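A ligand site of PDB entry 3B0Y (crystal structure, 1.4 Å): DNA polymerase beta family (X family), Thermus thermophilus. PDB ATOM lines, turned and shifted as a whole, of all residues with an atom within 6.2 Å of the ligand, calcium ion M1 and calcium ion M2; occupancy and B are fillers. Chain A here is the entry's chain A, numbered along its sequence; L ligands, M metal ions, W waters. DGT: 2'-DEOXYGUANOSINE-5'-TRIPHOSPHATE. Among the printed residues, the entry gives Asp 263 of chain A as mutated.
Of the 22 residues printed, 2 come within 4 Å of calcium ion M1. The nearest printed residue that does not touch calcium ion M1 is Leu 199 (4.3 Å).
Water W3 lies within hydrogen-bond range of NH2 of Arg 191 (2.8 Å) and O1B of the ligand (2.8 Å). Water W1 lies within hydrogen-bond range of the backbone NH of Asp 263 (2.8 Å) and a nitrogen (N2) of the ligand (3.2 Å). Water W9 bridges OG of Ser 266 (2.7 Å) and O of Tyr 258 (2.7 Å).
The side-chain carboxylate (OD2) of Asp 200 binds calcium ion M1. An oxygen (O1G) of the ligand binds calcium ion M1, at 2.3 Å. Calcium ion M1 is bound by an oxygen (O2B) of the ligand. OD1 of Asp 198 is bound to calcium ion M1 (2.4 Å). O1A of the ligand is bound to calcium ion M1 (2.4 Å). The backbone carbonyl oxygen (O) of Asp 198 is bound to calcium ion M1, at 2.4 Å. Water W7 is bound to calcium ion M1.
Three residues have an atom within 4 Å of calcium ion M2: Asp 198, Asp 200 and Asp 243. The nearest printed residue that does not touch calcium ion M2 is Leu 199 (5.2 Å).
OD2 of Asp 243 is bound to calcium ion M2, 2.3 Å away. OD1 of Asp 200 binds calcium ion M2, at 2.4 Å. Calcium ion M2 is bound by water W8, 2.4 Å away. Water W6 is bound to calcium ion M2 (2.4 Å). Calcium ion M2 is bound by OD2 of Asp 198, 2.5 Å away. OD1 of Asp 198 is bound to calcium ion M2 (2.5 Å). Calcium ion M2 is bound by an oxygen (O1A) of the ligand (2.5 Å). Calcium ion M2 has seven donor atoms within binding distance.
O of Ser 188 is in hydrogen-bond range of N of Lys 193 (3.2 Å). O of Asp 200 lies within hydrogen-bond range of N of Cys 186. The backbone carbonyl oxygen (O) of Leu 199 is in hydrogen-bond range of the backbone NH (N) of Asp 243, 2.8 Å away. The backbone carbonyl oxygen (O) of Thr 195 sits at hydrogen-bond distance from the guanidinium group (NH2) of Arg 157 (2.9 Å). The backbone NH (N) of Gly 187 lies within hydrogen-bond range of the backbone carbonyl oxygen (O) of Leu 259. O of Thr 260 is in hydrogen-bond range of NH1 of Arg 191 (2.8 Å). O of Ser 262 lies within hydrogen-bond range of OG of Ser 266 (3.4 Å). The side-chain hydroxyl of Thr 260 sits close to the side-chain sulfur of Cys 186 (3.7 Å).
Merely in contact with the ligand: Gly 187 (3.4 Å), Val 196 (3.7 Å), Tyr 258 (3.2 Å), Leu 259 (3.4 Å), Gly 261 (3.4 Å), Ser 262 (3.9 Å) and Asp 263 (3.5 Å). Hydrophobic or aromatic side chains that line the ligand: Tyr 258 and Leu 259. 14 residues have an atom within 4 Å of the ligand: Arg 157, Gly 187, Ser 188, Arg 191, Val 196, Gly 197, Asp 198, Asp 200, Tyr 258, Leu 259, Thr 260, Gly 261, Ser 262 and Asp 263. The nearest printed residue that does not touch the ligand is Thr 195 (4.5 Å).
N of Ser 188 sits close to O2B of the ligand (3.0 Å). The guanidinium group (NH2) of Arg 157 is in salt-bridge range of an oxygen (O3G) of the ligand, at 2.8 Å. O of Thr 260 sits at hydrogen-bond distance from O3' of the ligand (3.4 Å). O1B of the ligand is in salt-bridge range of NH1 of Arg 191, at 3.0 Å. The side-chain hydroxyl of Ser 188 is in hydrogen-bond range of an oxygen (O3G) of the ligand (2.6 Å). The backbone NH (N) of Gly 197 sits at hydrogen-bond distance from an oxygen (O3G) of the ligand (2.9 Å).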
ATOM      1  N   ARG A 157     -12.636  19.893 -15.091  1.00  0.00           N
ATOM      2  CA  ARG A 157     -12.704  18.990 -13.933  1.00  0.00           C
ATOM      3  C   ARG A 157     -14.167  18.789 -13.556  1.00  0.00           C
ATOM      4  O   ARG A 157     -15.017  19.656 -13.795  1.00  0.00           O
ATOM      5  CB  ARG A 157     -11.886  19.569 -12.777  1.00  0.00           C
ATOM      6  CG  ARG A 157     -10.454  19.906 -13.217  1.00  0.00           C
ATOM      7  CD  ARG A 157      -9.573  20.378 -12.079  1.00  0.00           C
ATOM      8  NE  ARG A 157      -9.309  19.341 -11.072  1.00  0.00           N
ATOM      9  CZ  ARG A 157      -8.391  18.387 -11.176  1.00  0.00           C
ATOM     10  NH1 ARG A 157      -7.571  18.343 -12.230  1.00  0.00           N
ATOM     11  NH2 ARG A 157      -8.252  17.517 -10.202  1.00  0.00           N
ATOM     12  N   CYS A 186      -7.213   4.732  -9.205  1.00  0.00           N
ATOM     13  CA  CYS A 186      -6.104   5.483  -8.611  1.00  0.00           C
ATOM     14  C   CYS A 186      -6.236   6.984  -8.916  1.00  0.00           C
ATOM     15  O   CYS A 186      -7.340   7.507  -8.841  1.00  0.00           O
ATOM     16  CB  CYS A 186      -4.761   4.891  -9.032  1.00  0.00           C
ATOM     17  SG  CYS A 186      -4.523   3.162  -8.498  1.00  0.00           S
ATOM     18  N   GLY A 187      -5.134   7.651  -9.232  1.00  0.00           N
ATOM     19  CA  GLY A 187      -5.116   9.088  -9.463  1.00  0.00           C
ATOM     20  C   GLY A 187      -5.731   9.888  -8.328  1.00  0.00           C
ATOM     21  O   GLY A 187      -5.818   9.468  -7.156  1.00  0.00           O
ATOM     22  N   SER A 188      -6.175  11.091  -8.681  1.00  0.00           N
ATOM     23  CA  SER A 188      -6.722  12.004  -7.670  1.00  0.00           C
ATOM     24  C   SER A 188      -8.023  11.528  -7.051  1.00  0.00           C
ATOM     25  O   SER A 188      -8.323  11.871  -5.895  1.00  0.00           O
ATOM     26  CB  SER A 188      -6.881  13.406  -8.263  1.00  0.00           C
ATOM     27  OG  SER A 188      -7.817  13.322  -9.335  1.00  0.00           O
ATOM     28  N   ALA A 189      -8.749  10.667  -7.756  1.00  0.00           N
ATOM     29  CA  ALA A 189      -9.964  10.095  -7.174  1.00  0.00           C
ATOM     30  C   ALA A 189      -9.634   9.278  -5.923  1.00  0.00           C
ATOM     31  O   ALA A 189     -10.353   9.313  -4.926  1.00  0.00           O
ATOM     32  CB  ALA A 189     -10.695   9.194  -8.174  1.00  0.00           C
ATOM     33  N   ARG A 191      -7.292   9.757  -3.930  1.00  0.00           N
ATOM     34  CA  ARG A 191      -6.895  10.725  -2.895  1.00  0.00           C
ATOM     35  C   ARG A 191      -8.098  11.555  -2.384  1.00  0.00           C
ATOM     36  O   ARG A 191      -7.911  12.394  -1.521  1.00  0.00           O
ATOM     37  CB  ARG A 191      -5.779  11.640  -3.389  1.00  0.00           C
ATOM     38  CG  ARG A 191      -4.598  10.894  -4.017  1.00  0.00           C
ATOM     39  CD  ARG A 191      -3.320  11.755  -4.071  1.00  0.00           C
ATOM     40  NE  ARG A 191      -3.576  13.044  -4.719  1.00  0.00           N
ATOM     41  CZ  ARG A 191      -3.535  13.273  -6.028  1.00  0.00           C
ATOM     42  NH1 ARG A 191      -3.272  12.296  -6.913  1.00  0.00           N
ATOM     43  NH2 ARG A 191      -3.780  14.505  -6.497  1.00  0.00           N
ATOM     44  N   LYS A 193      -9.716  13.898  -3.783  1.00  0.00           N
ATOM     45  CA  LYS A 193      -9.722  15.297  -4.237  1.00  0.00           C
ATOM     46  C   LYS A 193     -11.125  15.663  -4.683  1.00  0.00           C
ATOM     47  O   LYS A 193     -11.807  14.840  -5.312  1.00  0.00           O
ATOM     48  CB  LYS A 193      -8.712  15.447  -5.363  1.00  0.00           C
ATOM     49  CG  LYS A 193      -8.376  16.909  -5.655  1.00  0.00           C
ATOM     50  CD  LYS A 193      -7.314  16.969  -6.730  1.00  0.00           C
ATOM     51  CE  LYS A 193      -6.961  18.406  -7.091  1.00  0.00           C
ATOM     52  NZ  LYS A 193      -6.194  19.019  -5.974  1.00  0.00           N
ATOM     53  N   THR A 195     -12.435  17.653  -6.903  1.00  0.00           N
ATOM     54  CA  THR A 195     -12.674  17.681  -8.363  1.00  0.00           C
ATOM     55  C   THR A 195     -11.575  16.866  -8.976  1.00  0.00           C
ATOM     56  O   THR A 195     -10.447  16.831  -8.454  1.00  0.00           O
ATOM     57  CB  THR A 195     -12.726  19.081  -8.994  1.00  0.00           C
ATOM     58  OG1 THR A 195     -11.430  19.673  -8.962  1.00  0.00           O
ATOM     59  CG2 THR A 195     -13.744  19.967  -8.235  1.00  0.00           C
ATOM     60  N   VAL A 196     -11.903  16.209 -10.077  1.00  0.00           N
ATOM     61  CA  VAL A 196     -10.962  15.304 -10.745  1.00  0.00           C
ATOM     62  C   VAL A 196     -10.865  15.609 -12.220  1.00  0.00           C
ATOM     63  O   VAL A 196     -11.853  16.048 -12.848  1.00  0.00           O
ATOM     64  CB  VAL A 196     -11.299  13.818 -10.520  1.00  0.00           C
ATOM     65  CG1 VAL A 196     -11.214  13.509  -9.009  1.00  0.00           C
ATOM     66  CG2 VAL A 196     -12.679  13.482 -11.115  1.00  0.00           C
ATOM     67  N   GLY A 197      -9.693  15.361 -12.788  1.00  0.00           N
ATOM     68  CA  GLY A 197      -9.539  15.362 -14.245  1.00  0.00           C
ATOM     69  C   GLY A 197      -9.882  13.974 -14.752  1.00  0.00           C
ATOM     70  O   GLY A 197     -10.927  13.402 -14.425  1.00  0.00           O
ATOM     71  N   ASP A 198      -9.008  13.416 -15.569  1.00  0.00           N
ATOM     72  CA  ASP A 198      -9.264  12.070 -16.056  1.00  0.00           C
ATOM     73  C   ASP A 198      -9.230  11.038 -14.908  1.00  0.00           C
ATOM     74  O   ASP A 198      -8.697  11.322 -13.816  1.00  0.00           O
ATOM     75  CB  ASP A 198      -8.324  11.681 -17.220  1.00  0.00           C
ATOM     76  CG  ASP A 198      -6.876  11.545 -16.812  1.00  0.00           C
ATOM     77  OD1 ASP A 198      -6.534  11.440 -15.621  1.00  0.00           O
ATOM     78  OD2 ASP A 198      -6.017  11.515 -17.713  1.00  0.00           O
ATOM     79  N   LEU A 199      -9.809   9.870 -15.166  1.00  0.00           N
ATOM     80  CA  LEU A 199      -9.791   8.775 -14.191  1.00  0.00           C
ATOM     81  C   LEU A 199      -8.708   7.789 -14.585  1.00  0.00           C
ATOM     82  O   LEU A 199      -8.515   7.545 -15.754  1.00  0.00           O
ATOM     83  CB  LEU A 199     -11.147   8.075 -14.166  1.00  0.00           C
ATOM     84  CG  LEU A 199     -12.259   8.968 -13.604  1.00  0.00           C
ATOM     85  CD1 LEU A 199     -13.610   8.438 -13.978  1.00  0.00           C
ATOM     86  CD2 LEU A 199     -12.132   9.194 -12.125  1.00  0.00           C
ATOM     87  N   ASP A 200      -8.006   7.241 -13.598  1.00  0.00           N
ATOM     88  CA  ASP A 200      -6.827   6.415 -13.853  1.00  0.00           C
ATOM     89  C   ASP A 200      -7.002   5.083 -13.137  1.00  0.00           C
ATOM     90  O   ASP A 200      -7.290   5.066 -11.934  1.00  0.00           O
ATOM     91  CB  ASP A 200      -5.601   7.120 -13.252  1.00  0.00           C
ATOM     92  CG  ASP A 200      -5.476   8.517 -13.752  1.00  0.00           C
ATOM     93  OD1 ASP A 200      -4.903   8.696 -14.847  1.00  0.00           O
ATOM     94  OD2 ASP A 200      -5.995   9.439 -13.065  1.00  0.00           O
ATOM     95  N   ASP A 243      -7.625   6.632 -18.267  1.00  0.00           N
ATOM     96  CA  ASP A 243      -6.321   6.060 -18.500  1.00  0.00           C
ATOM     97  C   ASP A 243      -6.240   4.716 -17.775  1.00  0.00           C
ATOM     98  O   ASP A 243      -6.689   4.582 -16.634  1.00  0.00           O
ATOM     99  CB  ASP A 243      -5.238   6.948 -17.905  1.00  0.00           C
ATOM    100  CG  ASP A 243      -4.977   8.213 -18.700  1.00  0.00           C
ATOM    101  OD1 ASP A 243      -5.342   8.307 -19.873  1.00  0.00           O
ATOM    102  OD2 ASP A 243      -4.342   9.106 -18.111  1.00  0.00           O
ATOM    103  N   GLN A 257       1.171   2.889  -5.972  1.00  0.00           N
ATOM    104  CA  GLN A 257       1.787   4.117  -5.490  1.00  0.00           C
ATOM    105  C   GLN A 257       1.987   5.081  -6.680  1.00  0.00           C
ATOM    106  O   GLN A 257       1.620   6.280  -6.625  1.00  0.00           O
ATOM    107  CB  GLN A 257       3.099   3.797  -4.799  1.00  0.00           C
ATOM    108  CG  GLN A 257       3.678   4.991  -4.031  1.00  0.00           C
ATOM    109  CD  GLN A 257       4.324   6.014  -4.966  1.00  0.00           C
ATOM    110  OE1 GLN A 257       5.119   5.679  -5.846  1.00  0.00           O
ATOM    111  NE2 GLN A 257       3.966   7.276  -4.779  1.00  0.00           N
ATOM    112  N   TYR A 258       2.553   4.564  -7.770  1.00  0.00           N
ATOM    113  CA  TYR A 258       2.864   5.400  -8.927  1.00  0.00           C
ATOM    114  C   TYR A 258       1.610   6.114  -9.426  1.00  0.00           C
ATOM    115  O   TYR A 258       1.631   7.325  -9.695  1.00  0.00           O
ATOM    116  CB  TYR A 258       3.447   4.505 -10.032  1.00  0.00           C
ATOM    117  CG  TYR A 258       3.679   5.223 -11.331  1.00  0.00           C
ATOM    118  CD1 TYR A 258       4.891   5.848 -11.583  1.00  0.00           C
ATOM    119  CD2 TYR A 258       2.669   5.303 -12.280  1.00  0.00           C
ATOM    120  CE1 TYR A 258       5.103   6.526 -12.770  1.00  0.00           C
ATOM    121  CE2 TYR A 258       2.878   5.965 -13.485  1.00  0.00           C
ATOM    122  CZ  TYR A 258       4.079   6.586 -13.720  1.00  0.00           C
ATOM    123  OH  TYR A 258       4.287   7.275 -14.895  1.00  0.00           O
ATOM    124  N   LEU A 259       0.546   5.348  -9.636  1.00  0.00           N
ATOM    125  CA  LEU A 259      -0.619   5.888 -10.300  1.00  0.00           C
ATOM    126  C   LEU A 259      -1.517   6.721  -9.373  1.00  0.00           C
ATOM    127  O   LEU A 259      -2.418   7.400  -9.850  1.00  0.00           O
ATOM    128  CB  LEU A 259      -1.373   4.754 -11.001  1.00  0.00           C
ATOM    129  CG  LEU A 259      -2.333   5.239 -12.091  1.00  0.00           C
ATOM    130  CD1 LEU A 259      -1.681   6.125 -13.092  1.00  0.00           C
ATOM    131  CD2 LEU A 259      -3.090   4.098 -12.747  1.00  0.00           C
ATOM    132  N   THR A 260      -1.290   6.615  -8.063  1.00  0.00           N
ATOM    133  CA  THR A 260      -2.074   7.391  -7.097  1.00  0.00           C
ATOM    134  C   THR A 260      -1.464   8.763  -6.856  1.00  0.00           C
ATOM    135  O   THR A 260      -2.180   9.723  -6.589  1.00  0.00           O
ATOM    136  CB  THR A 260      -2.202   6.599  -5.769  1.00  0.00           C
ATOM    137  OG1 THR A 260      -2.937   5.391  -6.056  1.00  0.00           O
ATOM    138  CG2 THR A 260      -2.960   7.398  -4.694  1.00  0.00           C
ATOM    139  N   GLY A 261      -0.133   8.865  -6.939  1.00  0.00           N
ATOM    140  CA  GLY A 261       0.536  10.121  -6.686  1.00  0.00           C
ATOM    141  C   GLY A 261       0.172  10.674  -5.315  1.00  0.00           C
ATOM    142  O   GLY A 261      -0.004   9.918  -4.368  1.00  0.00           O
ATOM    143  N   SER A 262       0.022  11.994  -5.159  1.00  0.00           N
ATOM    144  CA  SER A 262       0.272  13.004  -6.181  1.00  0.00           C
ATOM    145  C   SER A 262       1.704  12.929  -6.692  1.00  0.00           C
ATOM    146  O   SER A 262       2.588  12.285  -6.084  1.00  0.00           O
ATOM    147  CB  SER A 262       0.038  14.365  -5.555  1.00  0.00           C
ATOM    148  OG  SER A 262       1.074  14.650  -4.615  1.00  0.00           O
ATOM    149  N   ASP A 263       1.963  13.626  -7.793  1.00  0.00           N
ATOM    150  CA  ASP A 263       3.298  13.701  -8.336  1.00  0.00           C
ATOM    151  C   ASP A 263       4.250  14.208  -7.241  1.00  0.00           C
ATOM    152  O   ASP A 263       5.339  13.660  -7.062  1.00  0.00           O
ATOM    153  CB  ASP A 263       3.297  14.636  -9.546  1.00  0.00           C
ATOM    154  CG  ASP A 263       4.603  14.624 -10.299  1.00  0.00           C
ATOM    155  OD1 ASP A 263       5.202  13.550 -10.488  1.00  0.00           O
ATOM    156  OD2 ASP A 263       5.017  15.726 -10.709  1.00  0.00           O
ATOM    157  N   SER A 266       5.123  11.426  -4.849  1.00  0.00           N
ATOM    158  CA  SER A 266       5.993  10.420  -5.454  1.00  0.00           C
ATOM    159  C   SER A 266       7.420  10.968  -5.590  1.00  0.00           C
ATOM    160  O   SER A 266       8.378  10.225  -5.409  1.00  0.00           O
ATOM    161  CB  SER A 266       5.462  10.034  -6.814  1.00  0.00           C
ATOM    162  OG  SER A 266       4.209   9.413  -6.676  1.00  0.00           O
HETATM  163  PG  DGT L   1      -6.066  15.006 -12.037  1.00  0.00           P
HETATM  164  O1G DGT L   1      -6.217  13.985 -13.140  1.00  0.00           O
HETATM  165  O2G DGT L   1      -5.605  16.373 -12.501  1.00  0.00           O
HETATM  166  O3G DGT L   1      -7.312  15.085 -11.166  1.00  0.00           O
HETATM  167  O3B DGT L   1      -4.919  14.468 -11.016  1.00  0.00           O
HETATM  168  PB  DGT L   1      -4.125  13.084 -11.010  1.00  0.00           P
HETATM  169  O1B DGT L   1      -3.278  13.058  -9.791  1.00  0.00           O
HETATM  170  O2B DGT L   1      -5.053  11.918 -11.283  1.00  0.00           O
HETATM  171  O3A DGT L   1      -3.104  13.235 -12.239  1.00  0.00           O
HETATM  172  PA  DGT L   1      -2.851  12.463 -13.626  1.00  0.00           P
HETATM  173  O1A DGT L   1      -4.106  11.797 -14.102  1.00  0.00           O
HETATM  174  O2A DGT L   1      -2.182  13.457 -14.528  1.00  0.00           O
HETATM  175  O5' DGT L   1      -1.757  11.398 -13.256  1.00  0.00           O
HETATM  176  C5' DGT L   1      -2.117  10.281 -12.419  1.00  0.00           C
HETATM  177  C4' DGT L   1      -0.959   9.957 -11.489  1.00  0.00           C
HETATM  178  O4' DGT L   1       0.150   9.584 -12.300  1.00  0.00           O
HETATM  179  C3' DGT L   1      -0.438  11.119 -10.643  1.00  0.00           C
HETATM  180  O3' DGT L   1      -1.137  11.274  -9.420  1.00  0.00           O
HETATM  181  C2' DGT L   1       1.009  10.717 -10.359  1.00  0.00           C
HETATM  182  C1' DGT L   1       1.380   9.864 -11.586  1.00  0.00           C
HETATM  183  N9  DGT L   1       2.291  10.603 -12.482  1.00  0.00           N
HETATM  184  C8  DGT L   1       3.284  10.070 -13.213  1.00  0.00           C
HETATM  185  N7  DGT L   1       3.909  11.034 -13.931  1.00  0.00           N
HETATM  186  C5  DGT L   1       3.320  12.209 -13.663  1.00  0.00           C
HETATM  187  C6  DGT L   1       3.493  13.625 -14.077  1.00  0.00           C
HETATM  188  O6  DGT L   1       4.383  13.955 -14.898  1.00  0.00           O
HETATM  189  N1  DGT L   1       2.668  14.552 -13.546  1.00  0.00           N
HETATM  190  C2  DGT L   1       1.691  14.252 -12.666  1.00  0.00           C
HETATM  191  N2  DGT L   1       0.888  15.235 -12.157  1.00  0.00           N
HETATM  192  N3  DGT L   1       1.497  12.975 -12.259  1.00  0.00           N
HETATM  193  C4  DGT L   1       2.258  11.941 -12.710  1.00  0.00           C
HETATM  194 CA    CA M   1      -6.368  11.686 -13.249  1.00  0.00          CA
HETATM  195 CA    CA M   2      -4.301  10.519 -16.242  1.00  0.00          CA
HETATM  196  O   HOH W   1       0.014  15.230  -9.085  1.00  0.00           O
HETATM  197  O   HOH W   2       0.334  12.932 -15.664  1.00  0.00           O
HETATM  198  O   HOH W   3      -2.723  15.637  -8.790  1.00  0.00           O
HETATM  199  O   HOH W   4      -4.072  17.418 -14.467  1.00  0.00           O
HETATM  200  O   HOH W   5      -6.363  14.803 -15.743  1.00  0.00           O
HETATM  201  O   HOH W   6      -2.052   9.659 -16.050  1.00  0.00           O
HETATM  202  O   HOH W   7      -7.974  11.462 -11.302  1.00  0.00           O
HETATM  203  O   HOH W   8      -3.094  12.391 -17.153  1.00  0.00           O
HETATM  204  O   HOH W   9       3.732   8.948  -9.272  1.00  0.00           O
HETATM  205  O   HOH W  10      -4.174  17.646 -10.399  1.00  0.00           O
HETATM  206  O   HOH W  11       0.515  10.189 -15.110  1.00  0.00           O
